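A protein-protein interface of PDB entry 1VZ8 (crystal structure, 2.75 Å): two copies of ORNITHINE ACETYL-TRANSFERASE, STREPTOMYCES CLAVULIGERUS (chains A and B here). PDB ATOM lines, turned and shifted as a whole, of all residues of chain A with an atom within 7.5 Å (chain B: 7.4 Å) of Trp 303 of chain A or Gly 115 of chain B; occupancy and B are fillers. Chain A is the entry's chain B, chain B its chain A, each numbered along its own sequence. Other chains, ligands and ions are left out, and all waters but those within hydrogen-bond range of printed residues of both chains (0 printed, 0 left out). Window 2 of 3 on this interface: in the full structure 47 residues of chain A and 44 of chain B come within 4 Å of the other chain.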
ATOM      1  N   VAL A 292      -0.685 -19.077   6.087  1.00  0.00           N
ATOM      2  CA  VAL A 292       0.694 -19.554   6.100  1.00  0.00           C
ATOM      3  C   VAL A 292       1.575 -18.343   6.429  1.00  0.00           C
ATOM      4  O   VAL A 292       2.378 -18.387   7.346  1.00  0.00           O
ATOM      5  CB  VAL A 292       1.122 -20.131   4.718  1.00  0.00           C
ATOM      6  CG1 VAL A 292       2.621 -20.344   4.691  1.00  0.00           C
ATOM      7  CG2 VAL A 292       0.424 -21.461   4.449  1.00  0.00           C
ATOM      8  N   ALA A 295       1.235 -17.130  10.146  1.00  0.00           N
ATOM      9  CA  ALA A 295       1.822 -18.113  11.058  1.00  0.00           C
ATOM     10  C   ALA A 295       3.356 -17.983  11.027  1.00  0.00           C
ATOM     11  O   ALA A 295       4.003 -17.919  12.078  1.00  0.00           O
ATOM     12  CB  ALA A 295       1.409 -19.525  10.662  1.00  0.00           C
ATOM     13  N   ASP A 300       5.540 -19.720  14.083  1.00  0.00           N
ATOM     14  CA  ASP A 300       4.786 -20.940  14.284  1.00  0.00           C
ATOM     15  C   ASP A 300       5.041 -21.878  13.116  1.00  0.00           C
ATOM     16  O   ASP A 300       4.714 -21.556  11.987  1.00  0.00           O
ATOM     17  CB  ASP A 300       3.290 -20.588  14.409  1.00  0.00           C
ATOM     18  CG  ASP A 300       2.388 -21.804  14.406  1.00  0.00           C
ATOM     19  OD1 ASP A 300       2.886 -22.909  14.687  1.00  0.00           O
ATOM     20  OD2 ASP A 300       1.172 -21.656  14.138  1.00  0.00           O
ATOM     21  N   PRO A 301       5.673 -23.037  13.369  1.00  0.00           N
ATOM     22  CA  PRO A 301       5.957 -24.008  12.303  1.00  0.00           C
ATOM     23  C   PRO A 301       4.693 -24.794  11.991  1.00  0.00           C
ATOM     24  O   PRO A 301       4.687 -26.026  12.000  1.00  0.00           O
ATOM     25  CB  PRO A 301       7.040 -24.881  12.916  1.00  0.00           C
ATOM     26  CG  PRO A 301       6.691 -24.868  14.353  1.00  0.00           C
ATOM     27  CD  PRO A 301       6.343 -23.425  14.618  1.00  0.00           C
ATOM     28  N   ASN A 302       3.623 -24.057  11.717  1.00  0.00           N
ATOM     29  CA  ASN A 302       2.316 -24.632  11.431  1.00  0.00           C
ATOM     30  C   ASN A 302       2.226 -25.488  10.163  1.00  0.00           C
ATOM     31  O   ASN A 302       1.842 -24.990   9.102  1.00  0.00           O
ATOM     32  CB  ASN A 302       1.291 -23.506  11.345  1.00  0.00           C
ATOM     33  CG  ASN A 302      -0.050 -23.892  11.923  1.00  0.00           C
ATOM     34  OD1 ASN A 302      -0.587 -24.973  11.635  1.00  0.00           O
ATOM     35  ND2 ASN A 302      -0.610 -23.004  12.743  1.00  0.00           N
ATOM     36  N   TRP A 303       2.562 -26.773  10.255  1.00  0.00           N
ATOM     37  CA  TRP A 303       2.467 -27.602   9.063  1.00  0.00           C
ATOM     38  C   TRP A 303       0.994 -27.761   8.681  1.00  0.00           C
ATOM     39  O   TRP A 303       0.649 -27.958   7.513  1.00  0.00           O
ATOM     40  CB  TRP A 303       3.130 -28.981   9.271  1.00  0.00           C
ATOM     41  CG  TRP A 303       2.593 -29.818  10.400  1.00  0.00           C
ATOM     42  CD1 TRP A 303       3.059 -29.858  11.682  1.00  0.00           C
ATOM     43  CD2 TRP A 303       1.493 -30.733  10.344  1.00  0.00           C
ATOM     44  NE1 TRP A 303       2.316 -30.739  12.428  1.00  0.00           N
ATOM     45  CE2 TRP A 303       1.350 -31.292  11.634  1.00  0.00           C
ATOM     46  CE3 TRP A 303       0.612 -31.133   9.330  1.00  0.00           C
ATOM     47  CZ2 TRP A 303       0.361 -32.236  11.942  1.00  0.00           C
ATOM     48  CZ3 TRP A 303      -0.379 -32.075   9.638  1.00  0.00           C
ATOM     49  CH2 TRP A 303      -0.493 -32.615  10.938  1.00  0.00           C
ATOM     50  N   GLY A 304       0.129 -27.656   9.677  1.00  0.00           N
ATOM     51  CA  GLY A 304      -1.289 -27.780   9.424  1.00  0.00           C
ATOM     52  C   GLY A 304      -1.727 -26.796   8.369  1.00  0.00           C
ATOM     53  O   GLY A 304      -2.375 -27.163   7.394  1.00  0.00           O
ATOM     54  N   ARG A 305      -1.373 -25.534   8.550  1.00  0.00           N
ATOM     55  CA  ARG A 305      -1.740 -24.532   7.565  1.00  0.00           C
ATOM     56  C   ARG A 305      -1.124 -24.818   6.195  1.00  0.00           C
ATOM     57  O   ARG A 305      -1.817 -24.707   5.183  1.00  0.00           O
ATOM     58  CB  ARG A 305      -1.334 -23.142   8.048  1.00  0.00           C
ATOM     59  CG  ARG A 305      -2.130 -22.694   9.255  1.00  0.00           C
ATOM     60  CD  ARG A 305      -1.908 -21.245   9.548  1.00  0.00           C
ATOM     61  NE  ARG A 305      -2.712 -20.832  10.685  1.00  0.00           N
ATOM     62  CZ  ARG A 305      -2.570 -19.673  11.315  1.00  0.00           C
ATOM     63  NH1 ARG A 305      -1.646 -18.811  10.908  1.00  0.00           N
ATOM     64  NH2 ARG A 305      -3.343 -19.379  12.351  1.00  0.00           N
ATOM     65  N   VAL A 306       0.160 -25.184   6.159  1.00  0.00           N
ATOM     66  CA  VAL A 306       0.820 -25.485   4.889  1.00  0.00           C
ATOM     67  C   VAL A 306       0.042 -26.571   4.164  1.00  0.00           C
ATOM     68  O   VAL A 306      -0.214 -26.476   2.957  1.00  0.00           O
ATOM     69  CB  VAL A 306       2.272 -25.997   5.082  1.00  0.00           C
ATOM     70  CG1 VAL A 306       2.775 -26.604   3.789  1.00  0.00           C
ATOM     71  CG2 VAL A 306       3.184 -24.864   5.497  1.00  0.00           C
ATOM     72  N   ALA A 307      -0.329 -27.608   4.907  1.00  0.00           N
ATOM     73  CA  ALA A 307      -1.071 -28.716   4.321  1.00  0.00           C
ATOM     74  C   ALA A 307      -2.308 -28.157   3.638  1.00  0.00           C
ATOM     75  O   ALA A 307      -2.542 -28.397   2.450  1.00  0.00           O
ATOM     76  CB  ALA A 307      -1.461 -29.701   5.389  1.00  0.00           C
ATOM     77  N   MET A 308      -3.080 -27.392   4.407  1.00  0.00           N
ATOM     78  CA  MET A 308      -4.305 -26.752   3.945  1.00  0.00           C
ATOM     79  C   MET A 308      -4.048 -26.010   2.645  1.00  0.00           C
ATOM     80  O   MET A 308      -4.799 -26.148   1.676  1.00  0.00           O
ATOM     81  CB  MET A 308      -4.802 -25.790   5.027  1.00  0.00           C
ATOM     82  CG  MET A 308      -6.088 -25.008   4.709  1.00  0.00           C
ATOM     83  SD  MET A 308      -5.853 -23.427   3.607  1.00  0.00           S
ATOM     84  CE  MET A 308      -4.909 -22.314   4.888  1.00  0.00           C
ATOM     85  N   ALA A 309      -2.981 -25.220   2.611  1.00  0.00           N
ATOM     86  CA  ALA A 309      -2.680 -24.485   1.397  1.00  0.00           C
ATOM     87  C   ALA A 309      -2.591 -25.471   0.249  1.00  0.00           C
ATOM     88  O   ALA A 309      -3.219 -25.290  -0.780  1.00  0.00           O
ATOM     89  CB  ALA A 309      -1.378 -23.720   1.541  1.00  0.00           C
ATOM     90  N   ILE A 310      -1.818 -26.531   0.425  1.00  0.00           N
ATOM     91  CA  ILE A 310      -1.699 -27.499  -0.642  1.00  0.00           C
ATOM     92  C   ILE A 310      -3.102 -27.931  -1.027  1.00  0.00           C
ATOM     93  O   ILE A 310      -3.474 -27.905  -2.202  1.00  0.00           O
ATOM     94  CB  ILE A 310      -0.900 -28.721  -0.196  1.00  0.00           C
ATOM     95  CG1 ILE A 310       0.431 -28.270   0.411  1.00  0.00           C
ATOM     96  CG2 ILE A 310      -0.658 -29.655  -1.398  1.00  0.00           C
ATOM     97  CD1 ILE A 310       1.284 -29.420   0.913  1.00  0.00           C
ATOM     98  N   ILE A 326       6.029 -32.652   4.425  1.00  0.00           N
ATOM     99  CA  ILE A 326       6.285 -31.226   4.590  1.00  0.00           C
ATOM    100  C   ILE A 326       7.428 -31.043   5.576  1.00  0.00           C
ATOM    101  O   ILE A 326       7.508 -31.740   6.596  1.00  0.00           O
ATOM    102  CB  ILE A 326       5.041 -30.488   5.164  1.00  0.00           C
ATOM    103  CG1 ILE A 326       3.807 -30.766   4.299  1.00  0.00           C
ATOM    104  CG2 ILE A 326       5.324 -29.001   5.274  1.00  0.00           C
ATOM    105  CD1 ILE A 326       2.505 -30.220   4.873  1.00  0.00           C
ATOM    106  N   ARG A 327       8.315 -30.105   5.282  1.00  0.00           N
ATOM    107  CA  ARG A 327       9.407 -29.870   6.186  1.00  0.00           C
ATOM    108  C   ARG A 327       9.743 -28.395   6.270  1.00  0.00           C
ATOM    109  O   ARG A 327       9.549 -27.640   5.316  1.00  0.00           O
ATOM    110  CB  ARG A 327      10.640 -30.663   5.741  1.00  0.00           C
ATOM    111  CG  ARG A 327      11.234 -30.194   4.428  1.00  0.00           C
ATOM    112  CD  ARG A 327      12.737 -30.383   4.433  1.00  0.00           C
ATOM    113  NE  ARG A 327      13.420 -29.421   3.571  1.00  0.00           N
ATOM    114  CZ  ARG A 327      13.253 -29.355   2.254  1.00  0.00           C
ATOM    115  NH1 ARG A 327      12.419 -30.204   1.653  1.00  0.00           N
ATOM    116  NH2 ARG A 327      13.912 -28.445   1.543  1.00  0.00           N
ATOM    117  N   PHE A 328      10.232 -27.998   7.439  1.00  0.00           N
ATOM    118  CA  PHE A 328      10.648 -26.633   7.710  1.00  0.00           C
ATOM    119  C   PHE A 328      12.143 -26.772   7.907  1.00  0.00           C
ATOM    120  O   PHE A 328      12.593 -27.513   8.783  1.00  0.00           O
ATOM    121  CB  PHE A 328       9.986 -26.131   8.978  1.00  0.00           C
ATOM    122  CG  PHE A 328       8.558 -25.728   8.791  1.00  0.00           C
ATOM    123  CD1 PHE A 328       8.239 -24.594   8.050  1.00  0.00           C
ATOM    124  CD2 PHE A 328       7.530 -26.468   9.370  1.00  0.00           C
ATOM    125  CE1 PHE A 328       6.927 -24.200   7.892  1.00  0.00           C
ATOM    126  CE2 PHE A 328       6.203 -26.082   9.218  1.00  0.00           C
ATOM    127  CZ  PHE A 328       5.901 -24.948   8.480  1.00  0.00           C
ATOM    128  N   VAL A 333       8.400 -32.326   9.371  1.00  0.00           N
ATOM    129  CA  VAL A 333       7.351 -32.302  10.391  1.00  0.00           C
ATOM    130  C   VAL A 333       6.013 -32.888   9.942  1.00  0.00           C
ATOM    131  O   VAL A 333       5.007 -32.748  10.633  1.00  0.00           O
ATOM    132  CB  VAL A 333       7.127 -30.874  10.895  1.00  0.00           C
ATOM    133  CG1 VAL A 333       8.405 -30.363  11.492  1.00  0.00           C
ATOM    134  CG2 VAL A 333       6.693 -29.970   9.751  1.00  0.00           C
ATOM    135  N   TYR A 334       6.009 -33.526   8.777  1.00  0.00           N
ATOM    136  CA  TYR A 334       4.812 -34.174   8.252  1.00  0.00           C
ATOM    137  C   TYR A 334       5.163 -35.227   7.196  1.00  0.00           C
ATOM    138  O   TYR A 334       5.873 -34.946   6.227  1.00  0.00           O
ATOM    139  CB  TYR A 334       3.839 -33.176   7.629  1.00  0.00           C
ATOM    140  CG  TYR A 334       2.595 -33.862   7.093  1.00  0.00           C
ATOM    141  CD1 TYR A 334       1.518 -34.153   7.925  1.00  0.00           C
ATOM    142  CD2 TYR A 334       2.519 -34.268   5.760  1.00  0.00           C
ATOM    143  CE1 TYR A 334       0.396 -34.829   7.444  1.00  0.00           C
ATOM    144  CE2 TYR A 334       1.410 -34.942   5.270  1.00  0.00           C
ATOM    145  CZ  TYR A 334       0.353 -35.221   6.111  1.00  0.00           C
ATOM    146  OH  TYR A 334      -0.746 -35.898   5.617  1.00  0.00           O
ATOM    147  N   PRO A 335       4.629 -36.445   7.348  1.00  0.00           N
ATOM    148  CA  PRO A 335       3.732 -36.879   8.425  1.00  0.00           C
ATOM    149  C   PRO A 335       4.328 -36.719   9.822  1.00  0.00           C
ATOM    150  O   PRO A 335       5.547 -36.704   9.994  1.00  0.00           O
ATOM    151  CB  PRO A 335       3.459 -38.343   8.078  1.00  0.00           C
ATOM    152  CG  PRO A 335       3.614 -38.379   6.589  1.00  0.00           C
ATOM    153  CD  PRO A 335       4.860 -37.538   6.394  1.00  0.00           C
ATOM    154  N   PRO A 336       3.468 -36.595  10.843  1.00  0.00           N
ATOM    155  CA  PRO A 336       3.907 -36.436  12.238  1.00  0.00           C
ATOM    156  C   PRO A 336       4.653 -37.676  12.756  1.00  0.00           C
ATOM    157  O   PRO A 336       4.689 -37.942  13.963  1.00  0.00           O
ATOM    158  CB  PRO A 336       2.592 -36.203  12.987  1.00  0.00           C
ATOM    159  CG  PRO A 336       1.688 -35.623  11.942  1.00  0.00           C
ATOM    160  CD  PRO A 336       2.005 -36.460  10.735  1.00  0.00           C
ATOM    161  N   ILE A 362      10.139 -23.822   3.471  1.00  0.00           N
ATOM    162  CA  ILE A 362       9.062 -24.790   3.527  1.00  0.00           C
ATOM    163  C   ILE A 362       9.289 -25.771   2.384  1.00  0.00           C
ATOM    164  O   ILE A 362       9.119 -25.428   1.218  1.00  0.00           O
ATOM    165  CB  ILE A 362       7.687 -24.110   3.355  1.00  0.00           C
ATOM    166  CG1 ILE A 362       7.541 -22.978   4.379  1.00  0.00           C
ATOM    167  CG2 ILE A 362       6.576 -25.145   3.501  1.00  0.00           C
ATOM    168  CD1 ILE A 362       6.205 -22.298   4.379  1.00  0.00           C
ATOM    169  N   PHE B  49      -6.693 -32.178   1.013  1.00  0.00           N
ATOM    170  CA  PHE B  49      -6.453 -32.598   2.377  1.00  0.00           C
ATOM    171  C   PHE B  49      -7.798 -32.691   3.093  1.00  0.00           C
ATOM    172  O   PHE B  49      -7.885 -32.458   4.289  1.00  0.00           O
ATOM    173  CB  PHE B  49      -5.558 -31.599   3.110  1.00  0.00           C
ATOM    174  CG  PHE B  49      -4.113 -32.012   3.192  1.00  0.00           C
ATOM    175  CD1 PHE B  49      -3.241 -31.779   2.134  1.00  0.00           C
ATOM    176  CD2 PHE B  49      -3.617 -32.622   4.340  1.00  0.00           C
ATOM    177  CE1 PHE B  49      -1.899 -32.145   2.229  1.00  0.00           C
ATOM    178  CE2 PHE B  49      -2.286 -32.987   4.439  1.00  0.00           C
ATOM    179  CZ  PHE B  49      -1.428 -32.749   3.386  1.00  0.00           C
ATOM    180  N   ASN B  75     -11.697 -28.818  16.783  1.00  0.00           N
ATOM    181  CA  ASN B  75     -10.798 -29.874  16.330  1.00  0.00           C
ATOM    182  C   ASN B  75     -11.414 -30.460  15.080  1.00  0.00           C
ATOM    183  O   ASN B  75     -12.496 -31.034  15.123  1.00  0.00           O
ATOM    184  CB  ASN B  75     -10.612 -30.969  17.378  1.00  0.00           C
ATOM    185  CG  ASN B  75      -9.560 -32.005  16.963  1.00  0.00           C
ATOM    186  OD1 ASN B  75      -9.361 -32.280  15.770  1.00  0.00           O
ATOM    187  ND2 ASN B  75      -8.897 -32.591  17.948  1.00  0.00           N
ATOM    188  N   ALA B  76     -10.714 -30.309  13.965  1.00  0.00           N
ATOM    189  CA  ALA B  76     -11.192 -30.786  12.676  1.00  0.00           C
ATOM    190  C   ALA B  76     -10.970 -32.270  12.369  1.00  0.00           C
ATOM    191  O   ALA B  76     -11.602 -32.802  11.462  1.00  0.00           O
ATOM    192  CB  ALA B  76     -10.563 -29.939  11.573  1.00  0.00           C
ATOM    193  N   ASN B  77     -10.090 -32.936  13.118  1.00  0.00           N
ATOM    194  CA  ASN B  77      -9.774 -34.348  12.865  1.00  0.00           C
ATOM    195  C   ASN B  77      -9.370 -34.465  11.399  1.00  0.00           C
ATOM    196  O   ASN B  77      -9.934 -35.250  10.625  1.00  0.00           O
ATOM    197  CB  ASN B  77     -10.968 -35.260  13.155  1.00  0.00           C
ATOM    198  CG  ASN B  77     -10.612 -36.736  13.041  1.00  0.00           C
ATOM    199  OD1 ASN B  77      -9.534 -37.158  13.451  1.00  0.00           O
ATOM    200  ND2 ASN B  77     -11.523 -37.527  12.496  1.00  0.00           N
ATOM    201  N   VAL B  78      -8.377 -33.653  11.049  1.00  0.00           N
ATOM    202  CA  VAL B  78      -7.839 -33.563   9.707  1.00  0.00           C
ATOM    203  C   VAL B  78      -6.348 -33.801   9.788  1.00  0.00           C
ATOM    204  O   VAL B  78      -5.665 -33.156  10.578  1.00  0.00           O
ATOM    205  CB  VAL B  78      -8.104 -32.152   9.125  1.00  0.00           C
ATOM    206  CG1 VAL B  78      -7.319 -31.949   7.837  1.00  0.00           C
ATOM    207  CG2 VAL B  78      -9.598 -31.971   8.866  1.00  0.00           C
ATOM    208  N   ALA B  79      -5.842 -34.717   8.966  1.00  0.00           N
ATOM    209  CA  ALA B  79      -4.414 -35.051   8.958  1.00  0.00           C
ATOM    210  C   ALA B  79      -4.069 -35.838  10.211  1.00  0.00           C
ATOM    211  O   ALA B  79      -2.954 -35.755  10.717  1.00  0.00           O
ATOM    212  CB  ALA B  79      -3.566 -33.781   8.896  1.00  0.00           C
ATOM    213  N   THR B  80      -5.051 -36.595  10.699  1.00  0.00           N
ATOM    214  CA  THR B  80      -4.913 -37.406  11.908  1.00  0.00           C
ATOM    215  C   THR B  80      -4.633 -38.874  11.585  1.00  0.00           C
ATOM    216  O   THR B  80      -4.651 -39.727  12.476  1.00  0.00           O
ATOM    217  CB  THR B  80      -6.193 -37.346  12.754  1.00  0.00           C
ATOM    218  OG1 THR B  80      -7.331 -37.518  11.895  1.00  0.00           O
ATOM    219  CG2 THR B  80      -6.274 -36.039  13.520  1.00  0.00           C
ATOM    220  N   GLY B  81      -4.397 -39.159  10.305  1.00  0.00           N
ATOM    221  CA  GLY B  81      -4.100 -40.512   9.876  1.00  0.00           C
ATOM    222  C   GLY B  81      -5.203 -41.535  10.058  1.00  0.00           C
ATOM    223  O   GLY B  81      -6.387 -41.193  10.180  1.00  0.00           O
ATOM    224  N   GLY B 112     -12.077 -27.021  13.141  1.00  0.00           N
ATOM    225  CA  GLY B 112     -11.128 -26.795  14.217  1.00  0.00           C
ATOM    226  C   GLY B 112      -9.646 -26.981  13.938  1.00  0.00           C
ATOM    227  O   GLY B 112      -9.169 -26.790  12.806  1.00  0.00           O
ATOM    228  N   VAL B 113      -8.913 -27.345  14.991  1.00  0.00           N
ATOM    229  CA  VAL B 113      -7.470 -27.547  14.907  1.00  0.00           C
ATOM    230  C   VAL B 113      -7.084 -28.772  14.089  1.00  0.00           C
ATOM    231  O   VAL B 113      -7.598 -29.872  14.282  1.00  0.00           O
ATOM    232  CB  VAL B 113      -6.836 -27.636  16.319  1.00  0.00           C
ATOM    233  CG1 VAL B 113      -5.460 -28.316  16.256  1.00  0.00           C
ATOM    234  CG2 VAL B 113      -6.684 -26.227  16.891  1.00  0.00           C
ATOM    235  N   ILE B 114      -6.164 -28.556  13.167  1.00  0.00           N
ATOM    236  CA  ILE B 114      -5.679 -29.607  12.298  1.00  0.00           C
ATOM    237  C   ILE B 114      -4.536 -30.405  12.956  1.00  0.00           C
ATOM    238  O   ILE B 114      -3.819 -29.883  13.808  1.00  0.00           O
ATOM    239  CB  ILE B 114      -5.204 -28.969  10.978  1.00  0.00           C
ATOM    240  CG1 ILE B 114      -6.415 -28.415  10.227  1.00  0.00           C
ATOM    241  CG2 ILE B 114      -4.392 -29.958  10.170  1.00  0.00           C
ATOM    242  CD1 ILE B 114      -6.067 -27.378   9.188  1.00  0.00           C
ATOM    243  N   GLY B 115      -4.390 -31.674  12.588  1.00  0.00           N
ATOM    244  CA  GLY B 115      -3.302 -32.468  13.131  1.00  0.00           C
ATOM    245  C   GLY B 115      -3.434 -33.123  14.496  1.00  0.00           C
ATOM    246  O   GLY B 115      -2.683 -34.053  14.782  1.00  0.00           O
ATOM    247  N   ARG B 116      -4.363 -32.662  15.334  1.00  0.00           N
ATOM    248  CA  ARG B 116      -4.543 -33.246  16.659  1.00  0.00           C
ATOM    249  C   ARG B 116      -5.671 -34.281  16.675  1.00  0.00           C
ATOM    250  O   ARG B 116      -6.711 -34.090  16.057  1.00  0.00           O
ATOM    251  CB  ARG B 116      -4.814 -32.148  17.686  1.00  0.00           C
ATOM    252  N   GLN B 117      -5.451 -35.378  17.394  1.00  0.00           N
ATOM    253  CA  GLN B 117      -6.426 -36.460  17.508  1.00  0.00           C
ATOM    254  C   GLN B 117      -7.600 -36.076  18.412  1.00  0.00           C
ATOM    255  O   GLN B 117      -7.475 -35.191  19.246  1.00  0.00           O
ATOM    256  CB  GLN B 117      -5.742 -37.709  18.071  1.00  0.00           C
ATOM    257  CG  GLN B 117      -4.567 -38.226  17.236  1.00  0.00           C
ATOM    258  CD  GLN B 117      -4.985 -38.832  15.900  1.00  0.00           C
ATOM    259  OE1 GLN B 117      -6.069 -39.412  15.764  1.00  0.00           O
ATOM    260  NE2 GLN B 117      -4.109 -38.720  14.911  1.00  0.00           N
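O of Val 78 of chain B sits at hydrogen-bond distance from N of Gly 115 of chain B (2.8 Å). N of Ile 326 of chain A is in hydrogen-bond range of O of Tyr 334 of chain A, at 2.9 Å. The side-chain amide oxygen (OD1) of Asn 302 of chain A sits close to the backbone NH (N) of Gly 304 of chain A.
Among the printed residues, pairs that only touch across the chains: Ala 307 of chain A with Phe 49 of chain B, Tyr 334 of chain A with Phe 49 of chain B, Trp 303 of chain A with Gly 115 of chain B, Trp 303 of chain A with Ala 79 of chain B and Gly 304 of chain A with Ile 114 of chain B.
Asn 302 of chain A touches none of the printed residues of chain B. Of chain B, only Ala 79 and Gly 115 come within 4 Å of Trp 303 of chain A. Of the printed residues of chain B, Ala 307 of chain A touches Phe 49. Of the printed residues of chain B, Tyr 334 of chain A touches Phe 49. Printed residues of chain A within 4 Å of Phe 49 of chain B: Ala 307 and Tyr 334. Of the printed residues of chain A, Ala 79 of chain B touches Trp 303 (3.7 Å). Of the printed residues of chain A, Ile 114 of chain B touches Gly 304 (3.9 Å). Printed residues of chain A within 4 Å of Gly 115 of chain B: Trp 303. The nearest residue of chain A that does not touch Gly 115 of chain B is Pro 336 of chain A (5.4 Å).
Among the printed residues, 5 pairs touch across the chains. Among the printed residues, no Asp or Glu carboxylate lies within 4 Å of a Lys or Arg side-chain nitrogen of the other chain.
No position is printed for both chains.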
